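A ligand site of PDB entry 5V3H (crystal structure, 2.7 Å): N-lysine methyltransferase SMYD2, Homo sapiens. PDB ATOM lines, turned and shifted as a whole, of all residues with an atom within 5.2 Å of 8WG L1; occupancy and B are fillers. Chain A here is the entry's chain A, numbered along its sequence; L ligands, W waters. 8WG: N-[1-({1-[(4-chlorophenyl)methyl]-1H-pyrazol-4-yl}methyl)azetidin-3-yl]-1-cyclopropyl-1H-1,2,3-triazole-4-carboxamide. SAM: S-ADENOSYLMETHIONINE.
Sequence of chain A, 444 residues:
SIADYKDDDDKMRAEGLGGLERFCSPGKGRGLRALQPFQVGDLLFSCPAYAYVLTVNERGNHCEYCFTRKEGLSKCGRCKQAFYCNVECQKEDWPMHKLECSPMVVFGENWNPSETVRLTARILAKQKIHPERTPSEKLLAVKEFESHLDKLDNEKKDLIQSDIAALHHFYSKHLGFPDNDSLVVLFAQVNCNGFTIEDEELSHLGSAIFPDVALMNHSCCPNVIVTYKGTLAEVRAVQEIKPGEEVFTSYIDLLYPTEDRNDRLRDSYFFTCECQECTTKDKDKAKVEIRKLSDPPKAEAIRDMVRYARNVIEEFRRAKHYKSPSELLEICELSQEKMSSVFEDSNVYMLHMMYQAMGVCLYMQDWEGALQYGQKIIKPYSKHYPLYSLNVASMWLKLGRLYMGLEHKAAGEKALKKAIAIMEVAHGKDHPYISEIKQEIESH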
ATOM      1  N   CYS A 192     -27.608  10.461   1.988  1.00  0.00           N
ATOM      2  CA  CYS A 192     -28.040   9.389   2.907  1.00  0.00           C
ATOM      3  C   CYS A 192     -26.928   8.927   3.860  1.00  0.00           C
ATOM      4  O   CYS A 192     -27.199   8.473   4.974  1.00  0.00           O
ATOM      5  CB  CYS A 192     -28.575   8.182   2.107  1.00  0.00           C
ATOM      6  SG  CYS A 192     -28.995   6.689   3.064  1.00  0.00           S
ATOM      7  N   ASN A 193     -25.662   9.014   3.402  1.00  0.00           N
ATOM      8  CA  ASN A 193     -24.510   8.475   4.170  1.00  0.00           C
ATOM      9  C   ASN A 193     -23.422   9.464   4.657  1.00  0.00           C
ATOM     10  O   ASN A 193     -22.531   9.069   5.428  1.00  0.00           O
ATOM     11  CB  ASN A 193     -23.874   7.358   3.360  1.00  0.00           C
ATOM     12  CG  ASN A 193     -24.822   6.186   3.131  1.00  0.00           C
ATOM     13  OD1 ASN A 193     -24.859   5.247   3.919  1.00  0.00           O
ATOM     14  ND2 ASN A 193     -25.608   6.250   2.046  1.00  0.00           N
ATOM     15  N   GLY A 194     -23.492  10.733   4.241  1.00  0.00           N
ATOM     16  CA  GLY A 194     -22.460  11.732   4.530  1.00  0.00           C
ATOM     17  C   GLY A 194     -22.443  12.292   5.944  1.00  0.00           C
ATOM     18  O   GLY A 194     -23.495  12.402   6.579  1.00  0.00           O
ATOM     19  N   PHE A 195     -21.244  12.662   6.409  1.00  0.00           N
ATOM     20  CA  PHE A 195     -21.026  13.216   7.750  1.00  0.00           C
ATOM     21  C   PHE A 195     -20.541  14.647   7.718  1.00  0.00           C
ATOM     22  O   PHE A 195     -19.837  15.037   6.797  1.00  0.00           O
ATOM     23  CB  PHE A 195     -20.000  12.382   8.494  1.00  0.00           C
ATOM     24  CG  PHE A 195     -20.568  11.125   9.057  1.00  0.00           C
ATOM     25  CD1 PHE A 195     -20.765  10.021   8.261  1.00  0.00           C
ATOM     26  CD2 PHE A 195     -20.956  11.074  10.396  1.00  0.00           C
ATOM     27  CE1 PHE A 195     -21.321   8.859   8.776  1.00  0.00           C
ATOM     28  CE2 PHE A 195     -21.515   9.924  10.923  1.00  0.00           C
ATOM     29  CZ  PHE A 195     -21.700   8.816  10.109  1.00  0.00           C
ATOM     30  N   THR A 196     -20.908  15.415   8.752  1.00  0.00           N
ATOM     31  CA  THR A 196     -20.297  16.734   9.036  1.00  0.00           C
ATOM     32  C   THR A 196     -19.311  16.624  10.211  1.00  0.00           C
ATOM     33  O   THR A 196     -19.437  15.729  11.055  1.00  0.00           O
ATOM     34  CB  THR A 196     -21.355  17.806   9.359  1.00  0.00           C
ATOM     35  OG1 THR A 196     -22.283  17.311  10.339  1.00  0.00           O
ATOM     36  CG2 THR A 196     -22.111  18.190   8.108  1.00  0.00           C
ATOM     37  N   GLU A 198     -17.612  18.998  13.286  1.00  0.00           N
ATOM     38  CA  GLU A 198     -17.637  20.232  14.077  1.00  0.00           C
ATOM     39  C   GLU A 198     -16.534  20.198  15.127  1.00  0.00           C
ATOM     40  O   GLU A 198     -16.024  19.135  15.473  1.00  0.00           O
ATOM     41  CB  GLU A 198     -19.001  20.455  14.757  1.00  0.00           C
ATOM     42  CG  GLU A 198     -20.218  20.451  13.806  1.00  0.00           C
ATOM     43  CD  GLU A 198     -20.787  19.055  13.494  1.00  0.00           C
ATOM     44  OE1 GLU A 198     -20.444  18.071  14.195  1.00  0.00           O
ATOM     45  OE2 GLU A 198     -21.587  18.934  12.545  1.00  0.00           O
ATOM     46  N   ASP A 199     -16.168  21.383  15.633  1.00  0.00           N
ATOM     47  CA  ASP A 199     -15.173  21.504  16.716  1.00  0.00           C
ATOM     48  C   ASP A 199     -15.834  21.410  18.090  1.00  0.00           C
ATOM     49  O   ASP A 199     -17.030  21.222  18.189  1.00  0.00           O
ATOM     50  CB  ASP A 199     -14.351  22.800  16.560  1.00  0.00           C
ATOM     51  CG  ASP A 199     -15.169  24.057  16.830  1.00  0.00           C
ATOM     52  OD1 ASP A 199     -16.345  23.977  17.240  1.00  0.00           O
ATOM     53  OD2 ASP A 199     -14.605  25.154  16.612  1.00  0.00           O
ATOM     54  N   GLU A 200     -15.050  21.576  19.147  1.00  0.00           N
ATOM     55  CA  GLU A 200     -15.555  21.419  20.533  1.00  0.00           C
ATOM     56  C   GLU A 200     -16.643  22.427  20.968  1.00  0.00           C
ATOM     57  O   GLU A 200     -17.389  22.132  21.892  1.00  0.00           O
ATOM     58  CB  GLU A 200     -14.393  21.346  21.554  1.00  0.00           C
ATOM     59  CG  GLU A 200     -13.808  22.682  22.045  1.00  0.00           C
ATOM     60  CD  GLU A 200     -12.778  23.306  21.113  1.00  0.00           C
ATOM     61  OE1 GLU A 200     -12.822  23.054  19.883  1.00  0.00           O
ATOM     62  OE2 GLU A 200     -11.915  24.065  21.626  1.00  0.00           O
ATOM     63  N   LEU A 202     -18.939  23.348  18.668  1.00  0.00           N
ATOM     64  CA  LEU A 202     -19.946  23.040  17.618  1.00  0.00           C
ATOM     65  C   LEU A 202     -19.945  23.922  16.342  1.00  0.00           C
ATOM     66  O   LEU A 202     -20.932  23.935  15.607  1.00  0.00           O
ATOM     67  CB  LEU A 202     -21.374  22.965  18.218  1.00  0.00           C
ATOM     68  CG  LEU A 202     -21.591  22.086  19.451  1.00  0.00           C
ATOM     69  CD1 LEU A 202     -23.006  22.274  19.978  1.00  0.00           C
ATOM     70  CD2 LEU A 202     -21.332  20.618  19.132  1.00  0.00           C
ATOM     71  N   ALA A 214     -21.115   4.324   8.571  1.00  0.00           N
ATOM     72  CA  ALA A 214     -22.452   4.449   8.004  1.00  0.00           C
ATOM     73  C   ALA A 214     -23.243   3.144   7.939  1.00  0.00           C
ATOM     74  O   ALA A 214     -24.423   3.171   7.592  1.00  0.00           O
ATOM     75  CB  ALA A 214     -22.385   5.089   6.620  1.00  0.00           C
ATOM     76  N   VAL A 226     -20.239   8.849  18.149  1.00  0.00           N
ATOM     77  CA  VAL A 226     -19.181   9.087  17.142  1.00  0.00           C
ATOM     78  C   VAL A 226     -18.398  10.365  17.463  1.00  0.00           C
ATOM     79  O   VAL A 226     -18.976  11.438  17.483  1.00  0.00           O
ATOM     80  CB  VAL A 226     -19.801   9.225  15.724  1.00  0.00           C
ATOM     81  CG1 VAL A 226     -18.769   9.685  14.690  1.00  0.00           C
ATOM     82  CG2 VAL A 226     -20.446   7.914  15.309  1.00  0.00           C
ATOM     83  N   THR A 227     -17.092  10.252  17.705  1.00  0.00           N
ATOM     84  CA  THR A 227     -16.252  11.445  17.876  1.00  0.00           C
ATOM     85  C   THR A 227     -15.152  11.451  16.820  1.00  0.00           C
ATOM     86  O   THR A 227     -14.983  10.473  16.079  1.00  0.00           O
ATOM     87  CB  THR A 227     -15.677  11.556  19.311  1.00  0.00           C
ATOM     88  OG1 THR A 227     -14.818  10.445  19.598  1.00  0.00           O
ATOM     89  CG2 THR A 227     -16.803  11.610  20.342  1.00  0.00           C
ATOM     90  N   TYR A 228     -14.435  12.575  16.756  1.00  0.00           N
ATOM     91  CA  TYR A 228     -13.358  12.764  15.777  1.00  0.00           C
ATOM     92  C   TYR A 228     -11.991  13.010  16.424  1.00  0.00           C
ATOM     93  O   TYR A 228     -11.902  13.640  17.475  1.00  0.00           O
ATOM     94  CB  TYR A 228     -13.713  13.922  14.852  1.00  0.00           C
ATOM     95  CG  TYR A 228     -15.014  13.727  14.098  1.00  0.00           C
ATOM     96  CD1 TYR A 228     -15.200  12.610  13.285  1.00  0.00           C
ATOM     97  CD2 TYR A 228     -16.049  14.649  14.204  1.00  0.00           C
ATOM     98  CE1 TYR A 228     -16.397  12.414  12.600  1.00  0.00           C
ATOM     99  CE2 TYR A 228     -17.245  14.464  13.518  1.00  0.00           C
ATOM    100  CZ  TYR A 228     -17.422  13.338  12.724  1.00  0.00           C
ATOM    101  OH  TYR A 228     -18.605  13.152  12.042  1.00  0.00           O
ATOM    102  N   SER A 250     -27.424   7.919  17.251  1.00  0.00           N
ATOM    103  CA  SER A 250     -28.443   8.886  16.765  1.00  0.00           C
ATOM    104  C   SER A 250     -27.875   9.704  15.611  1.00  0.00           C
ATOM    105  O   SER A 250     -26.728  10.073  15.627  1.00  0.00           O
ATOM    106  CB  SER A 250     -28.902   9.860  17.844  1.00  0.00           C
ATOM    107  OG  SER A 250     -29.668  10.917  17.273  1.00  0.00           O
ATOM    108  N   TYR A 251     -28.760  10.047  14.671  1.00  0.00           N
ATOM    109  CA  TYR A 251     -28.429  10.701  13.418  1.00  0.00           C
ATOM    110  C   TYR A 251     -28.740  12.173  13.571  1.00  0.00           C
ATOM    111  O   TYR A 251     -28.410  12.942  12.673  1.00  0.00           O
ATOM    112  CB  TYR A 251     -29.314  10.168  12.274  1.00  0.00           C
ATOM    113  CG  TYR A 251     -29.029   8.787  11.696  1.00  0.00           C
ATOM    114  CD1 TYR A 251     -28.108   7.910  12.273  1.00  0.00           C
ATOM    115  CD2 TYR A 251     -29.726   8.343  10.581  1.00  0.00           C
ATOM    116  CE1 TYR A 251     -27.865   6.657  11.730  1.00  0.00           C
ATOM    117  CE2 TYR A 251     -29.492   7.089  10.021  1.00  0.00           C
ATOM    118  CZ  TYR A 251     -28.569   6.242  10.594  1.00  0.00           C
ATOM    119  OH  TYR A 251     -28.335   4.991  10.056  1.00  0.00           O
ATOM    120  N   TYR A 269     -33.967  10.993   5.741  1.00  0.00           N
ATOM    121  CA  TYR A 269     -33.611   9.543   5.710  1.00  0.00           C
ATOM    122  C   TYR A 269     -34.727   8.529   5.331  1.00  0.00           C
ATOM    123  O   TYR A 269     -34.476   7.317   5.270  1.00  0.00           O
ATOM    124  CB  TYR A 269     -32.953   9.147   7.038  1.00  0.00           C
ATOM    125  CG  TYR A 269     -31.677   9.902   7.318  1.00  0.00           C
ATOM    126  CD1 TYR A 269     -30.512   9.613   6.625  1.00  0.00           C
ATOM    127  CD2 TYR A 269     -31.629  10.910   8.293  1.00  0.00           C
ATOM    128  CE1 TYR A 269     -29.328  10.312   6.879  1.00  0.00           C
ATOM    129  CE2 TYR A 269     -30.452  11.620   8.550  1.00  0.00           C
ATOM    130  CZ  TYR A 269     -29.302  11.312   7.855  1.00  0.00           C
ATOM    131  OH  TYR A 269     -28.138  11.991   8.099  1.00  0.00           O
ATOM    132  N   LEU A 390     -22.572  15.026  24.016  1.00  0.00           N
ATOM    133  CA  LEU A 390     -21.592  16.041  23.593  1.00  0.00           C
ATOM    134  C   LEU A 390     -22.134  17.482  23.576  1.00  0.00           C
ATOM    135  O   LEU A 390     -21.367  18.455  23.713  1.00  0.00           O
ATOM    136  CB  LEU A 390     -21.022  15.717  22.209  1.00  0.00           C
ATOM    137  CG  LEU A 390     -20.346  14.359  22.001  1.00  0.00           C
ATOM    138  CD1 LEU A 390     -20.065  14.131  20.537  1.00  0.00           C
ATOM    139  CD2 LEU A 390     -19.070  14.257  22.792  1.00  0.00           C
ATOM    140  N   ALA A 393     -21.766  18.527  27.083  1.00  0.00           N
ATOM    141  CA  ALA A 393     -20.348  18.721  27.342  1.00  0.00           C
ATOM    142  C   ALA A 393     -19.831  20.063  26.788  1.00  0.00           C
ATOM    143  O   ALA A 393     -19.111  20.739  27.509  1.00  0.00           O
ATOM    144  CB  ALA A 393     -19.526  17.569  26.788  1.00  0.00           C
ATOM    145  N   SER A 394     -20.202  20.437  25.559  1.00  0.00           N
ATOM    146  CA  SER A 394     -19.735  21.721  24.990  1.00  0.00           C
ATOM    147  C   SER A 394     -20.317  22.972  25.692  1.00  0.00           C
ATOM    148  O   SER A 394     -19.663  24.012  25.725  1.00  0.00           O
ATOM    149  CB  SER A 394     -19.956  21.823  23.474  1.00  0.00           C
ATOM    150  OG  SER A 394     -21.230  22.306  23.141  1.00  0.00           O
ATOM    151  N   LEU A 397     -18.278  23.526  28.684  1.00  0.00           N
ATOM    152  CA  LEU A 397     -17.028  24.057  28.131  1.00  0.00           C
ATOM    153  C   LEU A 397     -17.089  25.559  27.885  1.00  0.00           C
ATOM    154  O   LEU A 397     -16.168  26.302  28.231  1.00  0.00           O
ATOM    155  CB  LEU A 397     -16.713  23.328  26.814  1.00  0.00           C
ATOM    156  CG  LEU A 397     -15.275  23.001  26.479  1.00  0.00           C
ATOM    157  CD1 LEU A 397     -14.619  22.216  27.611  1.00  0.00           C
ATOM    158  CD2 LEU A 397     -15.234  22.207  25.178  1.00  0.00           C
ATOM    159  N   MET A 423     -16.279  13.858  28.538  1.00  0.00           N
ATOM    160  CA  MET A 423     -15.384  13.608  27.407  1.00  0.00           C
ATOM    161  C   MET A 423     -14.573  12.327  27.586  1.00  0.00           C
ATOM    162  O   MET A 423     -14.307  11.624  26.601  1.00  0.00           O
ATOM    163  CB  MET A 423     -14.477  14.823  27.155  1.00  0.00           C
ATOM    164  CG  MET A 423     -15.244  16.051  26.661  1.00  0.00           C
ATOM    165  SD  MET A 423     -14.341  17.600  26.805  1.00  0.00           S
ATOM    166  CE  MET A 423     -13.298  17.512  25.365  1.00  0.00           C
ATOM    167  N   HIS A 427     -14.754  10.547  24.082  1.00  0.00           N
ATOM    168  CA  HIS A 427     -13.514  10.718  23.313  1.00  0.00           C
ATOM    169  C   HIS A 427     -12.337   9.860  23.808  1.00  0.00           C
ATOM    170  O   HIS A 427     -11.244   9.893  23.209  1.00  0.00           O
ATOM    171  CB  HIS A 427     -13.042  12.183  23.376  1.00  0.00           C
ATOM    172  CG  HIS A 427     -14.011  13.175  22.804  1.00  0.00           C
ATOM    173  ND1 HIS A 427     -13.918  13.631  21.502  1.00  0.00           N
ATOM    174  CD2 HIS A 427     -15.042  13.840  23.361  1.00  0.00           C
ATOM    175  CE1 HIS A 427     -14.877  14.506  21.287  1.00  0.00           C
ATOM    176  NE2 HIS A 427     -15.571  14.655  22.398  1.00  0.00           N
ATOM    177  N   TYR A 433      -8.022  17.050  23.132  1.00  0.00           N
ATOM    178  CA  TYR A 433      -8.923  17.999  23.790  1.00  0.00           C
ATOM    179  C   TYR A 433      -8.802  17.990  25.329  1.00  0.00           C
ATOM    180  O   TYR A 433      -8.863  19.044  25.949  1.00  0.00           O
ATOM    181  CB  TYR A 433     -10.395  17.734  23.405  1.00  0.00           C
ATOM    182  CG  TYR A 433     -10.784  18.096  21.993  1.00  0.00           C
ATOM    183  CD1 TYR A 433     -10.387  19.305  21.422  1.00  0.00           C
ATOM    184  CD2 TYR A 433     -11.595  17.261  21.231  1.00  0.00           C
ATOM    185  CE1 TYR A 433     -10.753  19.639  20.125  1.00  0.00           C
ATOM    186  CE2 TYR A 433     -11.975  17.596  19.930  1.00  0.00           C
ATOM    187  CZ  TYR A 433     -11.552  18.787  19.392  1.00  0.00           C
ATOM    188  OH  TYR A 433     -11.916  19.143  18.115  1.00  0.00           O
HETATM  189  C2  8WG L   1     -17.013  18.360  22.399  1.00  0.00           C
HETATM  190  C3  8WG L   1     -15.898  18.083  21.607  1.00  0.00           C
HETATM  191  C4  8WG L   1     -16.025  17.942  20.231  1.00  0.00           C
HETATM  192  C5  8WG L   1     -17.270  18.054  19.627  1.00  0.00           C
HETATM  193  C6  8WG L   1     -17.373  17.905  18.124  1.00  0.00           C
HETATM  194  C8  8WG L   1     -19.560  17.200  17.134  1.00  0.00           C
HETATM  195 CL1  8WG L   1     -16.835  18.540  24.120  1.00  0.00          CL
HETATM  196  N7  8WG L   1     -18.336  16.923  17.615  1.00  0.00           N
HETATM  197  C9  8WG L   1     -20.136  16.054  16.715  1.00  0.00           C
HETATM  198  C10 8WG L   1     -21.520  15.958  16.122  1.00  0.00           C
HETATM  199  N11 8WG L   1     -21.497  15.862  14.651  1.00  0.00           N
HETATM  200  C12 8WG L   1     -22.852  15.745  14.078  1.00  0.00           C
HETATM  201  C13 8WG L   1     -22.255  14.840  13.000  1.00  0.00           C
HETATM  202  C14 8WG L   1     -21.216  14.534  14.093  1.00  0.00           C
HETATM  203  N15 8WG L   1     -23.058  13.660  12.636  1.00  0.00           N
HETATM  204  C16 8WG L   1     -23.456  13.384  11.370  1.00  0.00           C
HETATM  205  O17 8WG L   1     -23.174  14.122  10.433  1.00  0.00           O
HETATM  206  C18 8WG L   1     -24.216  12.159  11.079  1.00  0.00           C
HETATM  207  C19 8WG L   1     -24.270  11.595   9.856  1.00  0.00           C
HETATM  208  N20 8WG L   1     -25.025  10.498   9.949  1.00  0.00           N
HETATM  209  N21 8WG L   1     -25.436  10.398  11.281  1.00  0.00           N
HETATM  210  N22 8WG L   1     -24.946  11.397  11.928  1.00  0.00           N
HETATM  211  C23 8WG L   1     -25.295   9.612   8.822  1.00  0.00           C
HETATM  212  C24 8WG L   1     -25.623   8.158   9.182  1.00  0.00           C
HETATM  213  C25 8WG L   1     -26.719   9.085   8.649  1.00  0.00           C
HETATM  214  C26 8WG L   1     -19.208  15.024  16.959  1.00  0.00           C
HETATM  215  N27 8WG L   1     -18.141  15.546  17.495  1.00  0.00           N
HETATM  216  C28 8WG L   1     -18.380  18.339  20.404  1.00  0.00           C
HETATM  217  C29 8WG L   1     -18.253  18.480  21.780  1.00  0.00           C
HETATM  218  C2  8WG L   2     -22.327  16.530   2.873  1.00  0.00           C
HETATM  219  C3  8WG L   2     -23.571  16.341   2.292  1.00  0.00           C
HETATM  220  C4  8WG L   2     -24.624  15.850   3.055  1.00  0.00           C
HETATM  221  C5  8WG L   2     -24.438  15.546   4.389  1.00  0.00           C
HETATM  222  C6  8WG L   2     -25.588  15.021   5.218  1.00  0.00           C
HETATM  223  C8  8WG L   2     -25.548  15.310   7.710  1.00  0.00           C
HETATM  224 CL1  8WG L   2     -21.006  17.138   1.934  1.00  0.00          CL
HETATM  225  N7  8WG L   2     -25.722  15.785   6.457  1.00  0.00           N
HETATM  226  C9  8WG L   2     -25.761  16.327   8.574  1.00  0.00           C
HETATM  227  C10 8WG L   2     -25.662  16.223  10.076  1.00  0.00           C
HETATM  228  N11 8WG L   2     -26.633  17.090  10.755  1.00  0.00           N
HETATM  229  C12 8WG L   2     -28.048  16.704  10.577  1.00  0.00           C
HETATM  230  C13 8WG L   2     -28.233  16.740  12.106  1.00  0.00           C
HETATM  231  C14 8WG L   2     -26.710  16.782  12.197  1.00  0.00           C
HETATM  232  N15 8WG L   2     -28.874  17.972  12.614  1.00  0.00           N
HETATM  233  C16 8WG L   2     -30.000  17.931  13.368  1.00  0.00           C
HETATM  234  O17 8WG L   2     -30.541  16.878  13.640  1.00  0.00           O
HETATM  235  C18 8WG L   2     -30.636  19.163  13.884  1.00  0.00           C
HETATM  236  C19 8WG L   2     -30.224  20.451  13.710  1.00  0.00           C
HETATM  237  N20 8WG L   2     -31.103  21.236  14.369  1.00  0.00           N
HETATM  238  N21 8WG L   2     -32.062  20.389  14.938  1.00  0.00           N
HETATM  239  N22 8WG L   2     -31.756  19.181  14.632  1.00  0.00           N
HETATM  240  C23 8WG L   2     -31.067  22.700  14.449  1.00  0.00           C
HETATM  241  C24 8WG L   2     -32.348  23.401  14.887  1.00  0.00           C
HETATM  242  C25 8WG L   2     -31.152  23.327  15.844  1.00  0.00           C
HETATM  243  C26 8WG L   2     -26.078  17.465   7.834  1.00  0.00           C
HETATM  244  N27 8WG L   2     -26.053  17.151   6.560  1.00  0.00           N
HETATM  245  C28 8WG L   2     -23.194  15.735   4.970  1.00  0.00           C
HETATM  246  C29 8WG L   2     -22.136  16.227   4.216  1.00  0.00           C
HETATM  247  N   SAM L   3     -29.127   0.121   6.738  1.00  0.00           N
HETATM  248  CA  SAM L   3     -28.408   1.057   5.903  1.00  0.00           C
HETATM  249  C   SAM L   3     -27.933   0.336   4.671  1.00  0.00           C
HETATM  250  O   SAM L   3     -28.278   0.782   3.558  1.00  0.00           O
HETATM  251  OXT SAM L   3     -27.207  -0.671   4.805  1.00  0.00           O
HETATM  252  CB  SAM L   3     -27.221   1.685   6.639  1.00  0.00           C
HETATM  253  CG  SAM L   3     -27.630   2.939   7.407  1.00  0.00           C
HETATM  254  SD  SAM L   3     -27.817   4.234   6.392  1.00  0.00           S
HETATM  255  CE  SAM L   3     -26.631   5.347   6.726  1.00  0.00           C
HETATM  256  C5' SAM L   3     -29.287   4.987   6.631  1.00  0.00           C
HETATM  257  C4' SAM L   3     -30.511   4.179   6.203  1.00  0.00           C
HETATM  258  O4' SAM L   3     -30.758   3.041   7.039  1.00  0.00           O
HETATM  259  C3' SAM L   3     -31.765   5.006   6.286  1.00  0.00           C
HETATM  260  O3' SAM L   3     -32.001   5.734   5.081  1.00  0.00           O
HETATM  261  C2' SAM L   3     -32.846   3.993   6.582  1.00  0.00           C
HETATM  262  O2' SAM L   3     -33.373   3.421   5.374  1.00  0.00           O
HETATM  263  C1' SAM L   3     -32.138   2.906   7.358  1.00  0.00           C
HETATM  264  N9  SAM L   3     -32.376   3.010   8.830  1.00  0.00           N
HETATM  265  C8  SAM L   3     -31.508   3.446   9.752  1.00  0.00           C
HETATM  266  N7  SAM L   3     -32.045   3.406  10.999  1.00  0.00           N
HETATM  267  C5  SAM L   3     -33.285   2.921  10.883  1.00  0.00           C
HETATM  268  C6  SAM L   3     -34.397   2.597  11.811  1.00  0.00           C
HETATM  269  N6  SAM L   3     -34.281   2.815  13.143  1.00  0.00           N
HETATM  270  N1  SAM L   3     -35.545   2.104  11.283  1.00  0.00           N
HETATM  271  C2  SAM L   3     -35.683   1.888   9.953  1.00  0.00           C
HETATM  272  N3  SAM L   3     -34.702   2.146   9.054  1.00  0.00           N
HETATM  273  C4  SAM L   3     -33.506   2.650   9.453  1.00  0.00           C
HETATM  274  O   HOH W   1     -24.362   5.443  10.984  1.00  0.00           O
HETATM  275  O   HOH W   2     -14.916  15.353  18.010  1.00  0.00           O
HETATM  276  O   HOH W   3     -24.340   7.607  12.530  1.00  0.00           O
HETATM  277  O   HOH W   4     -27.381  13.261  10.197  1.00  0.00           O
HETATM  278  O   HOH W   5     -23.388  18.806  16.580  1.00  0.00           O
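The backbone carbonyl oxygen (O) of Tyr 269 sits at hydrogen-bond distance from an oxygen (O3') of SAM L3, at 2.9 Å. The side-chain sulfur of Cys 192 lies within hydrogen-bond range of an oxygen (O3') of SAM L3 (3.7 Å). O17 of 8WG L1 is in hydrogen-bond range of N of Thr 196 (3.1 Å). OG1 of Thr 196 is in hydrogen-bond range of O17 of 8WG L1 (3.3 Å). A nitrogen (N11) of 8WG L1 lies within salt-bridge range of the side-chain carboxylate (OE1) of Glu 198 (2.5 Å).
The side-chain carboxylate (OE2) of Glu 198 lies within hydrogen-bond range of the side-chain hydroxyl (OG1) of Thr 196, 2.8 Å away. The side-chain amide nitrogen of Asn 193 sits close to the side-chain sulfur of Cys 192, at 3.6 Å. The side-chain carboxylate of Asp 199 lies within hydrogen-bond range of the backbone NH of Leu 202 (3.0 Å). The side-chain hydroxyl of Tyr 228 is in hydrogen-bond range of the backbone carbonyl oxygen of Thr 196 (2.9 Å).
Cys 192 touches 8WG L1. Gly 194 touches 8WG L1 (O to C19, 3.5 Å). Phe 195 touches 8WG L1. O of Asp 199 touches C6 of 8WG L1, at 3.3 Å. CA of Glu 200 touches C3 of 8WG L1, at 3.5 Å. Leu 202 touches 8WG L1 (CD2 to C28, 3.9 Å). O of Val 226 touches C26 of 8WG L1, 3.6 Å away. OH of Tyr 228 touches C14 of 8WG L1, 3.6 Å away. Tyr 251 touches 8WG L1. Tyr 269 touches 8WG L1. Leu 390 touches 8WG L1 (O to C29, 3.7 Å). CB of Ala 393 touches CL1 of 8WG L1 (3.9 Å). SD of Met 423 touches CL1 of 8WG L1 (3.8 Å). His 427 touches 8WG L1. Hydrophobic or aromatic side chains that line 8WG L1: Phe 195, Leu 202, Tyr 251, Tyr 269, Leu 390, Ala 393, Met 423 and His 427. Of the 23 residues printed, 16 come within 4 Å of 8WG L1.
Water W2 lies within hydrogen-bond range of the backbone NH of Tyr 228 (3.1 Å) and a nitrogen (N27) of 8WG L1 (3.3 Å). Water W4 lies within hydrogen-bond range of the side-chain hydroxyl of Tyr 269 and the backbone carbonyl oxygen of Tyr 251.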
